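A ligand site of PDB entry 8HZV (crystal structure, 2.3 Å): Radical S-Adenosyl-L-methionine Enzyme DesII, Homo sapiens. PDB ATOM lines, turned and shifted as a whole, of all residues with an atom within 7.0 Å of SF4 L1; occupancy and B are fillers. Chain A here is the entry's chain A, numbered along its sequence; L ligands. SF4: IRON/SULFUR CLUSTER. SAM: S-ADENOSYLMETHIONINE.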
ATOM      1  N   THR A 140      15.920 -17.042 -24.517  1.00  0.00           N
ATOM      2  CA  THR A 140      15.002 -16.647 -23.454  1.00  0.00           C
ATOM      3  C   THR A 140      13.801 -17.577 -23.462  1.00  0.00           C
ATOM      4  O   THR A 140      13.718 -18.529 -24.253  1.00  0.00           O
ATOM      5  CB  THR A 140      14.566 -15.188 -23.628  1.00  0.00           C
ATOM      6  OG1 THR A 140      13.842 -14.772 -22.459  1.00  0.00           O
ATOM      7  CG2 THR A 140      13.669 -15.029 -24.840  1.00  0.00           C
ATOM      8  N   CYS A 141      12.861 -17.298 -22.562  1.00  0.00           N
ATOM      9  CA  CYS A 141      11.587 -17.989 -22.528  1.00  0.00           C
ATOM     10  C   CYS A 141      10.544 -17.077 -21.905  1.00  0.00           C
ATOM     11  O   CYS A 141      10.863 -16.252 -21.041  1.00  0.00           O
ATOM     12  CB  CYS A 141      11.653 -19.303 -21.745  1.00  0.00           C
ATOM     13  SG  CYS A 141      10.089 -20.164 -21.830  1.00  0.00           S
ATOM     14  N   MET A 142       9.292 -17.224 -22.349  1.00  0.00           N
ATOM     15  CA  MET A 142       8.190 -16.397 -21.858  1.00  0.00           C
ATOM     16  C   MET A 142       7.271 -17.145 -20.904  1.00  0.00           C
ATOM     17  O   MET A 142       6.239 -16.595 -20.495  1.00  0.00           O
ATOM     18  CB  MET A 142       7.393 -15.837 -23.040  1.00  0.00           C
ATOM     19  CG  MET A 142       6.525 -16.843 -23.778  1.00  0.00           C
ATOM     20  SD  MET A 142       7.457 -18.144 -24.607  1.00  0.00           S
ATOM     21  CE  MET A 142       8.232 -17.258 -25.947  1.00  0.00           C
ATOM     22  N   PHE A 143       7.616 -18.370 -20.520  1.00  0.00           N
ATOM     23  CA  PHE A 143       6.904 -19.113 -19.490  1.00  0.00           C
ATOM     24  C   PHE A 143       7.734 -19.151 -18.211  1.00  0.00           C
ATOM     25  O   PHE A 143       8.946 -18.933 -18.232  1.00  0.00           O
ATOM     26  CB  PHE A 143       6.592 -20.547 -19.935  1.00  0.00           C
ATOM     27  CG  PHE A 143       5.484 -20.647 -20.962  1.00  0.00           C
ATOM     28  CD1 PHE A 143       5.117 -21.883 -21.474  1.00  0.00           C
ATOM     29  CD2 PHE A 143       4.809 -19.519 -21.406  1.00  0.00           C
ATOM     30  CE1 PHE A 143       4.108 -21.995 -22.405  1.00  0.00           C
ATOM     31  CE2 PHE A 143       3.795 -19.626 -22.349  1.00  0.00           C
ATOM     32  CZ  PHE A 143       3.443 -20.867 -22.845  1.00  0.00           C
ATOM     33  N   ARG A 144       7.049 -19.417 -17.090  1.00  0.00           N
ATOM     34  CA  ARG A 144       7.703 -19.587 -15.793  1.00  0.00           C
ATOM     35  C   ARG A 144       7.071 -20.836 -15.148  1.00  0.00           C
ATOM     36  O   ARG A 144       6.293 -20.800 -14.194  1.00  0.00           O
ATOM     37  CB  ARG A 144       7.567 -18.323 -14.933  1.00  0.00           C
ATOM     38  CG  ARG A 144       7.754 -18.476 -13.420  1.00  0.00           C
ATOM     39  CD  ARG A 144       9.175 -18.826 -13.013  1.00  0.00           C
ATOM     40  NE  ARG A 144       9.523 -20.228 -13.219  1.00  0.00           N
ATOM     41  CZ  ARG A 144      10.779 -20.676 -13.251  1.00  0.00           C
ATOM     42  NH1 ARG A 144      11.782 -19.822 -13.082  1.00  0.00           N
ATOM     43  NH2 ARG A 144      11.028 -21.961 -13.443  1.00  0.00           N
ATOM     44  N   CYS A 145       7.394 -21.993 -15.721  1.00  0.00           N
ATOM     45  CA  CYS A 145       6.843 -23.261 -15.234  1.00  0.00           C
ATOM     46  C   CYS A 145       7.390 -23.566 -13.855  1.00  0.00           C
ATOM     47  O   CYS A 145       8.602 -23.470 -13.615  1.00  0.00           O
ATOM     48  CB  CYS A 145       7.176 -24.380 -16.210  1.00  0.00           C
ATOM     49  SG  CYS A 145       6.251 -24.330 -17.749  1.00  0.00           S
ATOM     50  N   HIS A 146       6.510 -23.959 -12.925  1.00  0.00           N
ATOM     51  CA  HIS A 146       6.947 -24.186 -11.551  1.00  0.00           C
ATOM     52  C   HIS A 146       7.899 -25.368 -11.439  1.00  0.00           C
ATOM     53  O   HIS A 146       8.699 -25.408 -10.491  1.00  0.00           O
ATOM     54  CB  HIS A 146       5.735 -24.374 -10.631  1.00  0.00           C
ATOM     55  CG  HIS A 146       4.849 -25.538 -10.988  1.00  0.00           C
ATOM     56  ND1 HIS A 146       5.100 -26.827 -10.558  1.00  0.00           N
ATOM     57  CD2 HIS A 146       3.708 -25.598 -11.721  1.00  0.00           C
ATOM     58  CE1 HIS A 146       4.155 -27.634 -11.015  1.00  0.00           C
ATOM     59  NE2 HIS A 146       3.298 -26.905 -11.726  1.00  0.00           N
ATOM     60  N   PHE A 147       7.865 -26.312 -12.368  1.00  0.00           N
ATOM     61  CA  PHE A 147       8.739 -27.477 -12.327  1.00  0.00           C
ATOM     62  C   PHE A 147      10.054 -27.293 -13.081  1.00  0.00           C
ATOM     63  O   PHE A 147      10.910 -28.186 -13.029  1.00  0.00           O
ATOM     64  CB  PHE A 147       8.012 -28.705 -12.891  1.00  0.00           C
ATOM     65  CG  PHE A 147       7.327 -28.456 -14.198  1.00  0.00           C
ATOM     66  CD1 PHE A 147       8.037 -28.506 -15.394  1.00  0.00           C
ATOM     67  CD2 PHE A 147       5.978 -28.158 -14.241  1.00  0.00           C
ATOM     68  CE1 PHE A 147       7.404 -28.265 -16.597  1.00  0.00           C
ATOM     69  CE2 PHE A 147       5.346 -27.917 -15.443  1.00  0.00           C
ATOM     70  CZ  PHE A 147       6.059 -27.963 -16.623  1.00  0.00           C
ATOM     71  N   CYS A 148      10.235 -26.177 -13.783  1.00  0.00           N
ATOM     72  CA  CYS A 148      11.470 -25.925 -14.510  1.00  0.00           C
ATOM     73  C   CYS A 148      12.496 -25.253 -13.601  1.00  0.00           C
ATOM     74  O   CYS A 148      12.161 -24.436 -12.741  1.00  0.00           O
ATOM     75  CB  CYS A 148      11.201 -25.049 -15.734  1.00  0.00           C
ATOM     76  SG  CYS A 148      12.694 -24.668 -16.665  1.00  0.00           S
ATOM     77  N   VAL A 149      13.772 -25.619 -13.812  1.00  0.00           N
ATOM     78  CA  VAL A 149      14.853 -25.071 -12.990  1.00  0.00           C
ATOM     79  C   VAL A 149      15.394 -23.753 -13.510  1.00  0.00           C
ATOM     80  O   VAL A 149      16.317 -23.187 -12.906  1.00  0.00           O
ATOM     81  CB  VAL A 149      16.014 -26.090 -12.873  1.00  0.00           C
ATOM     82  CG1 VAL A 149      15.553 -27.350 -12.141  1.00  0.00           C
ATOM     83  CG2 VAL A 149      16.562 -26.432 -14.243  1.00  0.00           C
ATOM     84  N   ARG A 150      14.844 -23.230 -14.604  1.00  0.00           N
ATOM     85  CA  ARG A 150      15.313 -21.952 -15.130  1.00  0.00           C
ATOM     86  C   ARG A 150      15.053 -20.830 -14.123  1.00  0.00           C
ATOM     87  O   ARG A 150      14.066 -20.839 -13.385  1.00  0.00           O
ATOM     88  CB  ARG A 150      14.652 -21.641 -16.474  1.00  0.00           C
ATOM     89  CG  ARG A 150      13.319 -20.923 -16.393  1.00  0.00           C
ATOM     90  CD  ARG A 150      12.865 -20.472 -17.776  1.00  0.00           C
ATOM     91  NE  ARG A 150      11.789 -19.482 -17.712  1.00  0.00           N
ATOM     92  CZ  ARG A 150      11.982 -18.181 -17.533  1.00  0.00           C
ATOM     93  NH1 ARG A 150      13.213 -17.703 -17.397  1.00  0.00           N
ATOM     94  NH2 ARG A 150      10.948 -17.353 -17.497  1.00  0.00           N
ATOM     95  N   GLY A 187      16.159 -27.458 -25.103  1.00  0.00           N
ATOM     96  CA  GLY A 187      16.739 -26.339 -24.418  1.00  0.00           C
ATOM     97  C   GLY A 187      16.786 -26.555 -22.928  1.00  0.00           C
ATOM     98  O   GLY A 187      16.228 -27.517 -22.378  1.00  0.00           O
ATOM     99  N   GLY A 188      17.528 -25.659 -22.289  1.00  0.00           N
ATOM    100  CA  GLY A 188      17.115 -25.165 -21.017  1.00  0.00           C
ATOM    101  C   GLY A 188      15.944 -24.257 -21.301  1.00  0.00           C
ATOM    102  O   GLY A 188      14.840 -24.475 -20.778  1.00  0.00           O
ATOM    103  N   LEU A 189      16.143 -23.284 -22.181  1.00  0.00           N
ATOM    104  CA  LEU A 189      15.129 -22.273 -22.485  1.00  0.00           C
ATOM    105  C   LEU A 189      14.324 -22.685 -23.727  1.00  0.00           C
ATOM    106  O   LEU A 189      14.317 -23.848 -24.120  1.00  0.00           O
ATOM    107  CB  LEU A 189      15.803 -20.907 -22.639  1.00  0.00           C
ATOM    108  CG  LEU A 189      16.483 -20.367 -21.374  1.00  0.00           C
ATOM    109  CD1 LEU A 189      16.820 -18.895 -21.492  1.00  0.00           C
ATOM    110  CD2 LEU A 189      15.620 -20.627 -20.145  1.00  0.00           C
ATOM    111  N   GLU A 190      13.639 -21.729 -24.354  1.00  0.00           N
ATOM    112  CA  GLU A 190      12.702 -22.023 -25.430  1.00  0.00           C
ATOM    113  C   GLU A 190      13.376 -21.814 -26.771  1.00  0.00           C
ATOM    114  O   GLU A 190      13.759 -20.679 -27.085  1.00  0.00           O
ATOM    115  CB  GLU A 190      11.464 -21.149 -25.307  1.00  0.00           C
ATOM    116  CG  GLU A 190      10.610 -21.060 -26.562  1.00  0.00           C
ATOM    117  CD  GLU A 190      10.071 -22.414 -26.994  1.00  0.00           C
ATOM    118  OE1 GLU A 190       9.600 -23.168 -26.115  1.00  0.00           O
ATOM    119  OE2 GLU A 190      10.119 -22.720 -28.199  1.00  0.00           O
ATOM    120  N   PRO A 191      13.520 -22.859 -27.596  1.00  0.00           N
ATOM    121  CA  PRO A 191      14.322 -22.712 -28.824  1.00  0.00           C
ATOM    122  C   PRO A 191      13.712 -21.797 -29.869  1.00  0.00           C
ATOM    123  O   PRO A 191      14.446 -21.205 -30.660  1.00  0.00           O
ATOM    124  CB  PRO A 191      14.456 -24.158 -29.337  1.00  0.00           C
ATOM    125  CG  PRO A 191      13.339 -24.889 -28.706  1.00  0.00           C
ATOM    126  CD  PRO A 191      13.099 -24.251 -27.369  1.00  0.00           C
ATOM    127  N   THR A 215       9.411 -27.811 -27.897  1.00  0.00           N
ATOM    128  CA  THR A 215       9.067 -26.404 -27.699  1.00  0.00           C
ATOM    129  C   THR A 215       7.754 -26.299 -26.953  1.00  0.00           C
ATOM    130  O   THR A 215       6.980 -27.258 -26.859  1.00  0.00           O
ATOM    131  CB  THR A 215       8.957 -25.673 -29.046  1.00  0.00           C
ATOM    132  OG1 THR A 215       8.417 -24.361 -28.840  1.00  0.00           O
ATOM    133  CG2 THR A 215       8.036 -26.438 -29.988  1.00  0.00           C
ATOM    134  N   ASN A 216       7.501 -25.103 -26.391  1.00  0.00           N
ATOM    135  CA  ASN A 216       6.190 -24.804 -25.844  1.00  0.00           C
ATOM    136  C   ASN A 216       5.215 -24.276 -26.891  1.00  0.00           C
ATOM    137  O   ASN A 216       4.025 -24.152 -26.604  1.00  0.00           O
ATOM    138  CB  ASN A 216       6.295 -23.807 -24.658  1.00  0.00           C
ATOM    139  CG  ASN A 216       6.824 -22.430 -25.056  1.00  0.00           C
ATOM    140  OD1 ASN A 216       6.583 -21.934 -26.155  1.00  0.00           O
ATOM    141  ND2 ASN A 216       7.551 -21.803 -24.133  1.00  0.00           N
ATOM    142  N   SER A 240       5.388 -29.265 -25.665  1.00  0.00           N
ATOM    143  CA  SER A 240       5.121 -29.516 -24.250  1.00  0.00           C
ATOM    144  C   SER A 240       3.775 -28.892 -23.881  1.00  0.00           C
ATOM    145  O   SER A 240       3.604 -27.678 -24.010  1.00  0.00           O
ATOM    146  CB  SER A 240       6.237 -28.946 -23.386  1.00  0.00           C
ATOM    147  OG  SER A 240       7.496 -29.430 -23.798  1.00  0.00           O
ATOM    148  N   TYR A 242       1.050 -27.980 -21.181  1.00  0.00           N
ATOM    149  CA  TYR A 242       1.035 -27.697 -19.749  1.00  0.00           C
ATOM    150  C   TYR A 242      -0.372 -27.500 -19.196  1.00  0.00           C
ATOM    151  O   TYR A 242      -0.515 -27.104 -18.032  1.00  0.00           O
ATOM    152  CB  TYR A 242       1.893 -26.467 -19.461  1.00  0.00           C
ATOM    153  CG  TYR A 242       3.344 -26.638 -19.890  1.00  0.00           C
ATOM    154  CD1 TYR A 242       4.031 -27.808 -19.597  1.00  0.00           C
ATOM    155  CD2 TYR A 242       4.004 -25.640 -20.577  1.00  0.00           C
ATOM    156  CE1 TYR A 242       5.343 -27.984 -19.983  1.00  0.00           C
ATOM    157  CE2 TYR A 242       5.329 -25.797 -20.971  1.00  0.00           C
ATOM    158  CZ  TYR A 242       5.999 -26.969 -20.661  1.00  0.00           C
ATOM    159  OH  TYR A 242       7.308 -27.136 -21.043  1.00  0.00           O
ATOM    160  N   THR A 252       0.119 -23.553 -14.209  1.00  0.00           N
ATOM    161  CA  THR A 252       1.382 -24.232 -14.459  1.00  0.00           C
ATOM    162  C   THR A 252       2.488 -23.253 -14.863  1.00  0.00           C
ATOM    163  O   THR A 252       3.576 -23.267 -14.277  1.00  0.00           O
ATOM    164  CB  THR A 252       1.191 -25.288 -15.541  1.00  0.00           C
ATOM    165  OG1 THR A 252       0.190 -26.230 -15.107  1.00  0.00           O
ATOM    166  CG2 THR A 252       2.480 -26.028 -15.795  1.00  0.00           C
ATOM    167  N   THR A 253       2.211 -22.385 -15.842  1.00  0.00           N
ATOM    168  CA  THR A 253       3.238 -21.518 -16.405  1.00  0.00           C
ATOM    169  C   THR A 253       3.239 -20.105 -15.847  1.00  0.00           C
ATOM    170  O   THR A 253       4.185 -19.355 -16.114  1.00  0.00           O
ATOM    171  CB  THR A 253       3.080 -21.434 -17.927  1.00  0.00           C
ATOM    172  OG1 THR A 253       2.030 -20.510 -18.241  1.00  0.00           O
ATOM    173  CG2 THR A 253       2.752 -22.806 -18.515  1.00  0.00           C
ATOM    174  N   PHE A 411      21.281 -23.974 -18.047  1.00  0.00           N
ATOM    175  CA  PHE A 411      20.442 -22.804 -17.867  1.00  0.00           C
ATOM    176  C   PHE A 411      21.305 -21.626 -17.460  1.00  0.00           C
ATOM    177  O   PHE A 411      22.180 -21.762 -16.598  1.00  0.00           O
ATOM    178  CB  PHE A 411      19.363 -23.037 -16.796  1.00  0.00           C
ATOM    179  CG  PHE A 411      18.313 -24.049 -17.193  1.00  0.00           C
ATOM    180  CD1 PHE A 411      18.572 -25.406 -17.124  1.00  0.00           C
ATOM    181  CD2 PHE A 411      17.065 -23.637 -17.601  1.00  0.00           C
ATOM    182  CE1 PHE A 411      17.604 -26.331 -17.467  1.00  0.00           C
ATOM    183  CE2 PHE A 411      16.085 -24.553 -17.943  1.00  0.00           C
ATOM    184  CZ  PHE A 411      16.356 -25.904 -17.878  1.00  0.00           C
HETATM  185 FE1  SF4 L   1       8.507 -24.026 -19.146  1.00  0.00          FE
HETATM  186 FE2  SF4 L   1      11.139 -24.091 -18.691  1.00  0.00          FE
HETATM  187 FE3  SF4 L   1      10.113 -22.158 -20.211  1.00  0.00          FE
HETATM  188 FE4  SF4 L   1      10.220 -24.731 -21.150  1.00  0.00          FE
HETATM  189  S1  SF4 L   1      12.014 -23.379 -20.642  1.00  0.00           S
HETATM  190  S2  SF4 L   1       8.423 -23.288 -21.254  1.00  0.00           S
HETATM  191  S3  SF4 L   1       9.835 -25.873 -19.277  1.00  0.00           S
HETATM  192  S4  SF4 L   1       9.713 -22.419 -18.042  1.00  0.00           S
HETATM  193  N   SAM L   2      10.830 -24.237 -23.522  1.00  0.00           N
HETATM  194  CA  SAM L   2      10.803 -25.470 -24.288  1.00  0.00           C
HETATM  195  C   SAM L   2       9.672 -26.394 -23.806  1.00  0.00           C
HETATM  196  O   SAM L   2       9.207 -27.280 -24.529  1.00  0.00           O
HETATM  197  OXT SAM L   2       9.169 -26.286 -22.690  1.00  0.00           O
HETATM  198  CB  SAM L   2      12.162 -26.168 -24.180  1.00  0.00           C
HETATM  199  CG  SAM L   2      12.038 -27.581 -23.656  1.00  0.00           C
HETATM  200  SD  SAM L   2      13.122 -28.056 -22.288  1.00  0.00           S
HETATM  201  CE  SAM L   2      12.374 -27.435 -20.760  1.00  0.00           C
HETATM  202  C5' SAM L   2      12.939 -29.874 -22.339  1.00  0.00           C
HETATM  203  C4' SAM L   2      11.692 -30.619 -21.835  1.00  0.00           C
HETATM  204  O4' SAM L   2      11.807 -30.924 -20.466  1.00  0.00           O
HETATM  205  C3' SAM L   2      10.330 -29.956 -22.031  1.00  0.00           C
HETATM  206  O3' SAM L   2       9.516 -30.808 -22.784  1.00  0.00           O
HETATM  207  C2' SAM L   2       9.766 -29.801 -20.629  1.00  0.00           C
HETATM  208  O2' SAM L   2       8.372 -30.032 -20.614  1.00  0.00           O
HETATM  209  C1' SAM L   2      10.528 -30.869 -19.868  1.00  0.00           C
HETATM  210  N9  SAM L   2      10.723 -30.619 -18.437  1.00  0.00           N
HETATM  211  C8  SAM L   2      11.318 -29.533 -17.857  1.00  0.00           C
HETATM  212  N7  SAM L   2      11.318 -29.728 -16.511  1.00  0.00           N
HETATM  213  C5  SAM L   2      10.750 -30.927 -16.240  1.00  0.00           C
HETATM  214  C6  SAM L   2      10.501 -31.601 -15.052  1.00  0.00           C
HETATM  215  N6  SAM L   2      10.855 -31.073 -13.890  1.00  0.00           N
HETATM  216  N1  SAM L   2       9.894 -32.840 -15.090  1.00  0.00           N
HETATM  217  C2  SAM L   2       9.528 -33.392 -16.299  1.00  0.00           C
HETATM  218  N3  SAM L   2       9.775 -32.709 -17.482  1.00  0.00           N
HETATM  219  C4  SAM L   2      10.383 -31.493 -17.446  1.00  0.00           C
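N of Cys 145 lies close to S4 of SF4 L1 (3.3 Å). SG of Cys 145 binds FE1 of SF4 L1. S3 of SF4 L1 sits close to OH of Tyr 242 (3.3 Å). OE1 of Glu 190 lies close to N of SAM L2 (3.1 Å). ND2 of Asn 216 lies close to S2 of SF4 L1 (3.4 Å). The guanidinium group (NE) of Arg 150 sits close to a sulfur (S4) of SF4 L1. N of Thr 215 sits close to O of SAM L2, 3.4 Å away. The side-chain hydroxyl (OG) of Ser 240 lies within hydrogen-bond range of an oxygen (O3') of SAM L2 (2.6 Å). The backbone NH of Asn 216 sits at hydrogen-bond distance from an oxygen (O) of SAM L2. SG of Cys 141 is bound to FE3 of SF4 L1, at 2.6 Å. An oxygen (O2') of SAM L2 sits at hydrogen-bond distance from the side-chain hydroxyl (OH) of Tyr 242, 3.1 Å away. The side-chain sulfur (SG) of Cys 148 binds an iron atom (FE2) of SF4 L1, at 2.6 Å. A nitrogen (N6) of SAM L2 sits at hydrogen-bond distance from the backbone carbonyl oxygen (O) of Phe 147 (3.0 Å).
The side-chain sulfur of Cys 141 lies close to the backbone NH of Phe 143, 3.3 Å away. The backbone carbonyl oxygen of Phe 143 sits at hydrogen-bond distance from the guanidinium group of Arg 150 (2.7 Å). N of Asn 216 lies within hydrogen-bond range of OE1 of Glu 190 (2.9 Å). The backbone carbonyl oxygen (O) of Tyr 242 is in hydrogen-bond range of the side-chain hydroxyl (OG1) of Thr 252 (3.1 Å). O of Arg 150 sits at hydrogen-bond distance from NH1 of Arg 144, 2.5 Å away. The backbone NH (N) of Arg 150 sits close to the side-chain sulfur (SG) of Cys 148 (3.3 Å). The side-chain amide nitrogen (ND2) of Asn 216 is in hydrogen-bond range of the side-chain sulfur (SD) of Met 142 (3.7 Å). The side-chain sulfur of Cys 141 lies close to the side-chain amide nitrogen of Asn 216.
O of Phe 143 sits close to S4 of SF4 L1 (3.6 Å). The backbone carbonyl oxygen (O) of Gly 188 lies close to a sulfur (S1) of SF4 L1 (3.0 Å). Leu 189 touches SF4 L1 (CA to S1, 3.8 Å). Hydrophobic or aromatic side chains within 4 Å of SF4 L1: Phe 143 and Tyr 242. Of the 23 residues printed, 9 come within 4 Å of SF4 L1.
FE4 of SF4 L1 is bound by OXT of SAM L2, at 2.4 Å.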
